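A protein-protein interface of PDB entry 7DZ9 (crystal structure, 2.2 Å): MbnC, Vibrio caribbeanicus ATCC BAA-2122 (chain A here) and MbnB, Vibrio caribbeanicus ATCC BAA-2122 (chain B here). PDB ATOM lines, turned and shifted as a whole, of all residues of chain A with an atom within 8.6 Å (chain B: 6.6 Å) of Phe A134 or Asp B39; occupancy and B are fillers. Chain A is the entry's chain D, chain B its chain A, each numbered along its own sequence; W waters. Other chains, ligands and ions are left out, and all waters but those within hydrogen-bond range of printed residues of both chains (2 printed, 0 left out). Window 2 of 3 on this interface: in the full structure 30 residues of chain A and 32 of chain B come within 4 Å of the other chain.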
ATOM      1  N   GLN A 113     -13.953  -4.148  21.186  1.00  0.00           N
ATOM      2  CA  GLN A 113     -12.519  -4.376  21.275  1.00  0.00           C
ATOM      3  C   GLN A 113     -12.125  -5.632  22.044  1.00  0.00           C
ATOM      4  O   GLN A 113     -10.976  -6.074  21.910  1.00  0.00           O
ATOM      5  CB  GLN A 113     -11.850  -3.156  21.915  1.00  0.00           C
ATOM      6  CG  GLN A 113     -12.061  -1.872  21.110  1.00  0.00           C
ATOM      7  CD  GLN A 113     -11.487  -0.648  21.799  1.00  0.00           C
ATOM      8  OE1 GLN A 113     -10.942  -0.746  22.894  1.00  0.00           O
ATOM      9  NE2 GLN A 113     -11.597   0.510  21.155  1.00  0.00           N
ATOM     10  N   LYS A 131      -8.390  -6.612  20.705  1.00  0.00           N
ATOM     11  CA  LYS A 131      -7.923  -6.293  19.362  1.00  0.00           C
ATOM     12  C   LYS A 131      -6.786  -5.274  19.414  1.00  0.00           C
ATOM     13  O   LYS A 131      -6.674  -4.482  20.356  1.00  0.00           O
ATOM     14  CB  LYS A 131      -9.076  -5.742  18.524  1.00  0.00           C
ATOM     15  CG  LYS A 131     -10.175  -6.774  18.252  1.00  0.00           C
ATOM     16  CD  LYS A 131     -11.322  -6.129  17.513  1.00  0.00           C
ATOM     17  CE  LYS A 131     -12.404  -7.147  17.219  1.00  0.00           C
ATOM     18  NZ  LYS A 131     -13.622  -6.476  16.721  1.00  0.00           N
ATOM     19  N   SER A 132      -5.931  -5.297  18.394  1.00  0.00           N
ATOM     20  CA  SER A 132      -4.963  -4.220  18.248  1.00  0.00           C
ATOM     21  C   SER A 132      -5.685  -2.878  18.179  1.00  0.00           C
ATOM     22  O   SER A 132      -6.698  -2.740  17.486  1.00  0.00           O
ATOM     23  CB  SER A 132      -4.122  -4.416  16.994  1.00  0.00           C
ATOM     24  OG  SER A 132      -3.365  -3.243  16.747  1.00  0.00           O
ATOM     25  N   LEU A 133      -5.176  -1.899  18.922  1.00  0.00           N
ATOM     26  CA  LEU A 133      -5.721  -0.548  18.935  1.00  0.00           C
ATOM     27  C   LEU A 133      -4.796   0.460  18.268  1.00  0.00           C
ATOM     28  O   LEU A 133      -5.186   1.618  18.096  1.00  0.00           O
ATOM     29  CB  LEU A 133      -6.022  -0.104  20.375  1.00  0.00           C
ATOM     30  CG  LEU A 133      -6.951  -1.035  21.165  1.00  0.00           C
ATOM     31  CD1 LEU A 133      -7.194  -0.530  22.587  1.00  0.00           C
ATOM     32  CD2 LEU A 133      -8.265  -1.170  20.407  1.00  0.00           C
ATOM     33  N   PHE A 134      -3.604   0.041  17.848  1.00  0.00           N
ATOM     34  CA  PHE A 134      -2.641   0.925  17.205  1.00  0.00           C
ATOM     35  C   PHE A 134      -1.893   0.127  16.141  1.00  0.00           C
ATOM     36  O   PHE A 134      -1.645  -1.070  16.309  1.00  0.00           O
ATOM     37  CB  PHE A 134      -1.673   1.533  18.233  1.00  0.00           C
ATOM     38  CG  PHE A 134      -2.330   2.472  19.223  1.00  0.00           C
ATOM     39  CD1 PHE A 134      -2.508   3.816  18.917  1.00  0.00           C
ATOM     40  CD2 PHE A 134      -2.766   2.008  20.463  1.00  0.00           C
ATOM     41  CE1 PHE A 134      -3.106   4.678  19.825  1.00  0.00           C
ATOM     42  CE2 PHE A 134      -3.364   2.872  21.382  1.00  0.00           C
ATOM     43  CZ  PHE A 134      -3.535   4.210  21.055  1.00  0.00           C
ATOM     44  N   ALA A 135      -1.551   0.807  15.039  1.00  0.00           N
ATOM     45  CA  ALA A 135      -1.095   0.135  13.821  1.00  0.00           C
ATOM     46  C   ALA A 135       0.042  -0.862  14.076  1.00  0.00           C
ATOM     47  O   ALA A 135       0.067  -1.952  13.486  1.00  0.00           O
ATOM     48  CB  ALA A 135      -0.667   1.172  12.783  1.00  0.00           C
ATOM     49  N   GLN A 136       1.000  -0.520  14.929  1.00  0.00           N
ATOM     50  CA  GLN A 136       2.155  -1.400  15.101  1.00  0.00           C
ATOM     51  C   GLN A 136       2.095  -2.247  16.366  1.00  0.00           C
ATOM     52  O   GLN A 136       3.091  -2.889  16.729  1.00  0.00           O
ATOM     53  CB  GLN A 136       3.443  -0.595  15.073  1.00  0.00           C
ATOM     54  CG  GLN A 136       3.685   0.093  13.750  1.00  0.00           C
ATOM     55  CD  GLN A 136       5.163   0.407  13.539  1.00  0.00           C
ATOM     56  OE1 GLN A 136       5.551   1.571  13.480  1.00  0.00           O
ATOM     57  NE2 GLN A 136       5.992  -0.641  13.429  1.00  0.00           N
ATOM     58  N   GLU A 137       0.945  -2.323  17.013  1.00  0.00           N
ATOM     59  CA  GLU A 137       0.827  -3.065  18.257  1.00  0.00           C
ATOM     60  C   GLU A 137       0.072  -4.365  18.028  1.00  0.00           C
ATOM     61  O   GLU A 137      -0.981  -4.364  17.383  1.00  0.00           O
ATOM     62  CB  GLU A 137       0.117  -2.231  19.317  1.00  0.00           C
ATOM     63  CG  GLU A 137       0.084  -2.962  20.632  1.00  0.00           C
ATOM     64  CD  GLU A 137       0.153  -2.030  21.799  1.00  0.00           C
ATOM     65  OE1 GLU A 137      -0.915  -1.463  22.155  1.00  0.00           O
ATOM     66  OE2 GLU A 137       1.280  -1.862  22.334  1.00  0.00           O
ATOM     67  N   PHE A 138       0.602  -5.461  18.568  1.00  0.00           N
ATOM     68  CA  PHE A 138      -0.081  -6.745  18.475  1.00  0.00           C
ATOM     69  C   PHE A 138      -1.385  -6.753  19.269  1.00  0.00           C
ATOM     70  O   PHE A 138      -1.551  -6.028  20.254  1.00  0.00           O
ATOM     71  CB  PHE A 138       0.811  -7.875  18.987  1.00  0.00           C
ATOM     72  CG  PHE A 138       1.788  -8.370  17.957  1.00  0.00           C
ATOM     73  CD1 PHE A 138       3.043  -7.780  17.833  1.00  0.00           C
ATOM     74  CD2 PHE A 138       1.442  -9.400  17.098  1.00  0.00           C
ATOM     75  CE1 PHE A 138       3.945  -8.214  16.875  1.00  0.00           C
ATOM     76  CE2 PHE A 138       2.343  -9.843  16.142  1.00  0.00           C
ATOM     77  CZ  PHE A 138       3.603  -9.241  16.034  1.00  0.00           C
ATOM     78  N   ARG A 139      -2.325  -7.571  18.798  1.00  0.00           N
ATOM     79  CA  ARG A 139      -3.451  -8.003  19.613  1.00  0.00           C
ATOM     80  C   ARG A 139      -2.941  -8.567  20.932  1.00  0.00           C
ATOM     81  O   ARG A 139      -1.864  -9.166  20.994  1.00  0.00           O
ATOM     82  CB  ARG A 139      -4.273  -9.087  18.876  1.00  0.00           C
ATOM     83  CG  ARG A 139      -3.441 -10.360  18.576  1.00  0.00           C
ATOM     84  CD  ARG A 139      -3.866 -11.602  19.358  1.00  0.00           C
ATOM     85  NE  ARG A 139      -3.038 -12.764  19.033  1.00  0.00           N
ATOM     86  CZ  ARG A 139      -1.795 -12.971  19.468  1.00  0.00           C
ATOM     87  NH1 ARG A 139      -1.213 -12.084  20.264  1.00  0.00           N
ATOM     88  NH2 ARG A 139      -1.134 -14.062  19.091  1.00  0.00           N
ATOM     89  N   GLN B  10       0.675  -7.297  12.007  1.00  0.00           N
ATOM     90  CA  GLN B  10       1.916  -6.862  12.630  1.00  0.00           C
ATOM     91  C   GLN B  10       3.081  -7.826  12.411  1.00  0.00           C
ATOM     92  O   GLN B  10       4.234  -7.406  12.534  1.00  0.00           O
ATOM     93  CB  GLN B  10       1.694  -6.637  14.137  1.00  0.00           C
ATOM     94  CG  GLN B  10       0.805  -5.398  14.463  1.00  0.00           C
ATOM     95  CD  GLN B  10      -0.681  -5.594  14.086  1.00  0.00           C
ATOM     96  OE1 GLN B  10      -1.312  -6.572  14.479  1.00  0.00           O
ATOM     97  NE2 GLN B  10      -1.231  -4.653  13.326  1.00  0.00           N
ATOM     98  N   PHE B  35      -8.199  -3.788  10.665  1.00  0.00           N
ATOM     99  CA  PHE B  35      -7.797  -2.550  11.324  1.00  0.00           C
ATOM    100  C   PHE B  35      -9.003  -1.772  11.846  1.00  0.00           C
ATOM    101  O   PHE B  35      -8.917  -0.557  12.060  1.00  0.00           O
ATOM    102  CB  PHE B  35      -6.980  -1.679  10.368  1.00  0.00           C
ATOM    103  CG  PHE B  35      -5.726  -2.336   9.869  1.00  0.00           C
ATOM    104  CD1 PHE B  35      -5.755  -3.162   8.752  1.00  0.00           C
ATOM    105  CD2 PHE B  35      -4.510  -2.118  10.508  1.00  0.00           C
ATOM    106  CE1 PHE B  35      -4.583  -3.766   8.277  1.00  0.00           C
ATOM    107  CE2 PHE B  35      -3.331  -2.714  10.043  1.00  0.00           C
ATOM    108  CZ  PHE B  35      -3.364  -3.539   8.929  1.00  0.00           C
ATOM    109  N   THR B  37     -10.580  -1.472  14.656  1.00  0.00           N
ATOM    110  CA  THR B  37     -10.452  -0.734  15.911  1.00  0.00           C
ATOM    111  C   THR B  37      -9.083  -0.075  16.052  1.00  0.00           C
ATOM    112  O   THR B  37      -8.629   0.186  17.172  1.00  0.00           O
ATOM    113  CB  THR B  37     -10.716  -1.637  17.112  1.00  0.00           C
ATOM    114  OG1 THR B  37      -9.754  -2.695  17.122  1.00  0.00           O
ATOM    115  CG2 THR B  37     -12.097  -2.226  17.032  1.00  0.00           C
ATOM    116  N   THR B  38      -8.405   0.175  14.940  1.00  0.00           N
ATOM    117  CA  THR B  38      -7.075   0.764  14.951  1.00  0.00           C
ATOM    118  C   THR B  38      -7.162   2.286  14.881  1.00  0.00           C
ATOM    119  O   THR B  38      -7.910   2.839  14.068  1.00  0.00           O
ATOM    120  CB  THR B  38      -6.262   0.235  13.769  1.00  0.00           C
ATOM    121  OG1 THR B  38      -6.307  -1.192  13.782  1.00  0.00           O
ATOM    122  CG2 THR B  38      -4.823   0.713  13.858  1.00  0.00           C
ATOM    123  N   ASP B  39      -6.383   2.951  15.719  1.00  0.00           N
ATOM    124  CA  ASP B  39      -6.270   4.404  15.667  1.00  0.00           C
ATOM    125  C   ASP B  39      -5.803   4.859  14.280  1.00  0.00           C
ATOM    126  O   ASP B  39      -4.737   4.455  13.811  1.00  0.00           O
ATOM    127  CB  ASP B  39      -5.307   4.864  16.762  1.00  0.00           C
ATOM    128  CG  ASP B  39      -5.044   6.354  16.725  1.00  0.00           C
ATOM    129  OD1 ASP B  39      -5.812   7.105  17.343  1.00  0.00           O
ATOM    130  OD2 ASP B  39      -4.055   6.767  16.081  1.00  0.00           O
ATOM    131  N   VAL B  40      -6.621   5.690  13.622  1.00  0.00           N
ATOM    132  CA  VAL B  40      -6.365   6.075  12.240  1.00  0.00           C
ATOM    133  C   VAL B  40      -5.077   6.883  12.132  1.00  0.00           C
ATOM    134  O   VAL B  40      -4.291   6.689  11.194  1.00  0.00           O
ATOM    135  CB  VAL B  40      -7.551   6.862  11.675  1.00  0.00           C
ATOM    136  CG1 VAL B  40      -7.424   6.990  10.174  1.00  0.00           C
ATOM    137  CG2 VAL B  40      -8.839   6.149  11.991  1.00  0.00           C
ATOM    138  N   ASP B  41      -4.803   7.762  13.105  1.00  0.00           N
ATOM    139  CA  ASP B  41      -3.557   8.514  13.085  1.00  0.00           C
ATOM    140  C   ASP B  41      -2.344   7.596  13.175  1.00  0.00           C
ATOM    141  O   ASP B  41      -1.344   7.832  12.493  1.00  0.00           O
ATOM    142  CB  ASP B  41      -3.550   9.533  14.214  1.00  0.00           C
ATOM    143  CG  ASP B  41      -4.540  10.652  13.971  1.00  0.00           C
ATOM    144  OD1 ASP B  41      -4.736  11.020  12.786  1.00  0.00           O
ATOM    145  OD2 ASP B  41      -5.145  11.130  14.954  1.00  0.00           O
ATOM    146  N   SER B  42      -2.406   6.540  14.003  1.00  0.00           N
ATOM    147  CA  SER B  42      -1.311   5.564  14.019  1.00  0.00           C
ATOM    148  C   SER B  42      -1.119   4.916  12.652  1.00  0.00           C
ATOM    149  O   SER B  42       0.003   4.562  12.294  1.00  0.00           O
ATOM    150  CB  SER B  42      -1.533   4.496  15.091  1.00  0.00           C
ATOM    151  OG  SER B  42      -2.463   3.494  14.684  1.00  0.00           O
ATOM    152  N   ILE B  43      -2.200   4.693  11.906  1.00  0.00           N
ATOM    153  CA  ILE B  43      -2.070   4.147  10.559  1.00  0.00           C
ATOM    154  C   ILE B  43      -1.381   5.158   9.650  1.00  0.00           C
ATOM    155  O   ILE B  43      -0.470   4.818   8.888  1.00  0.00           O
ATOM    156  CB  ILE B  43      -3.453   3.773  10.000  1.00  0.00           C
ATOM    157  CG1 ILE B  43      -3.993   2.493  10.646  1.00  0.00           C
ATOM    158  CG2 ILE B  43      -3.393   3.666   8.480  1.00  0.00           C
ATOM    159  CD1 ILE B  43      -5.411   2.179  10.209  1.00  0.00           C
ATOM    160  N   LYS B  44      -1.830   6.415   9.704  1.00  0.00           N
ATOM    161  CA  LYS B  44      -1.221   7.463   8.892  1.00  0.00           C
ATOM    162  C   LYS B  44       0.248   7.650   9.251  1.00  0.00           C
ATOM    163  O   LYS B  44       1.086   7.839   8.362  1.00  0.00           O
ATOM    164  CB  LYS B  44      -1.991   8.773   9.057  1.00  0.00           C
ATOM    165  CG  LYS B  44      -3.374   8.750   8.425  1.00  0.00           C
ATOM    166  CD  LYS B  44      -4.097  10.085   8.621  1.00  0.00           C
ATOM    167  CE  LYS B  44      -5.496  10.078   8.005  1.00  0.00           C
ATOM    168  NZ  LYS B  44      -6.299  11.313   8.304  1.00  0.00           N
ATOM    169  N   LEU B  79     -13.417   4.749   7.842  1.00  0.00           N
ATOM    170  CA  LEU B  79     -12.016   4.584   7.462  1.00  0.00           C
ATOM    171  C   LEU B  79     -11.755   5.040   6.025  1.00  0.00           C
ATOM    172  O   LEU B  79     -10.659   5.528   5.716  1.00  0.00           O
ATOM    173  CB  LEU B  79     -11.608   3.124   7.648  1.00  0.00           C
ATOM    174  CG  LEU B  79     -11.395   2.715   9.112  1.00  0.00           C
ATOM    175  CD1 LEU B  79     -11.394   1.213   9.258  1.00  0.00           C
ATOM    176  CD2 LEU B  79     -10.093   3.311   9.661  1.00  0.00           C
HETATM  177  O   HOH W   1      -7.801  -2.988  14.691  1.00  0.00           O
HETATM  178  O   HOH W   2      -3.751  -2.405  14.212  1.00  0.00           O
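The side-chain hydroxyl of Thr B38 lies close to the backbone carbonyl oxygen of Phe B35, 3.2 Å away.
The backbone NH (N) of Asp B41 sits at hydrogen-bond distance from the side-chain carboxylate (OD2) of Asp B39 (3.2 Å).
O of Asp B39 lies within hydrogen-bond range of OG of Ser B42 (2.6 Å).
N of Lys A131 lies within hydrogen-bond range of O of Gln A113 (2.9 Å).
OG of Ser A132 is in hydrogen-bond range of O of Phe A134 (2.8 Å).
OG of Ser A132 lies within hydrogen-bond range of O of Glu A137 (2.7 Å).
The side-chain amide nitrogen of Gln B10 lies within hydrogen-bond range of the backbone carbonyl oxygen of Ala A135 (3.0 Å).
The backbone carbonyl oxygen (O) of Ser A132 sits at hydrogen-bond distance from the side-chain hydroxyl (OG1) of Thr B37 (3.1 Å).
N of Asp B39 sits at hydrogen-bond distance from O of Leu A133 (3.0 Å).
N of Ala A135 is in hydrogen-bond range of OG of Ser B42 (2.9 Å).
Of chain B, only Thr B38 (3.8 Å), Asp B39 (3.7 Å) and Ser B42 (3.6 Å) come within 4 Å of Phe A134.
Of the printed residues of chain A, Asp B39 touches Leu A133 (3.0 Å) and Phe A134 (3.7 Å).
Of the printed residues of chain A, Gln B10 touches Ala A135, Gln A136, Glu A137 and Phe A138.
Printed residues of chain B within 4 Å of Lys A131: Thr B37.
Printed residues of chain A within 4 Å of Thr B38: Leu A133, Phe A134 and Ala A135.
Asp B41 touches none of the printed residues of chain A.
Phe B35 touches none of the printed residues of chain A.
The nearest residue of chain A that does not touch Asp B39 is Ala A135 (5.0 Å).
Water W1 lies within hydrogen-bond range of OG1 of Thr B38 (2.5 Å), O of Ser A132 (3.0 Å) and OG1 of Thr B37 (3.1 Å).
Water W2 lies within hydrogen-bond range of OG of Ser A132 (2.7 Å), OG1 of Thr B38 (2.9 Å), O of Phe A134 (3.3 Å) and NE2 of Gln B10 (3.5 Å).
Among the printed residues, merely in contact across the chains: Lys A131 with Thr B37 (3.4 Å), Leu A133 with Thr B37 (3.5 Å), Ala A135 with Thr B38 (3.5 Å), Glu A137 with Gln B10 (3.5 Å), Phe A134 with Ser B42 (3.6 Å), Phe A134 with Asp B39 (3.7 Å), Phe A138 with Gln B10 (3.7 Å), Phe A134 with Thr B38 (3.8 Å), Leu A133 with Thr B38 (3.8 Å), Gln A136 with Gln B10 (3.9 Å) and Ala A135 with Ile B43 (3.9 Å).
Along chain B the printed residues that touch a printed residue of chain A span positions 10 to 43.
Printed residues of chain A that touch a printed residue of chain B: Lys A131, Ser A132, Leu A133, Phe A134, Ala A135, Gln A136, Glu A137 and Phe A138.
Among the printed residues, 15 pairs touch across the chains.
Among the printed residues, no Asp or Glu carboxylate lies within 4 Å of a Lys or Arg side-chain nitrogen of the other chain.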
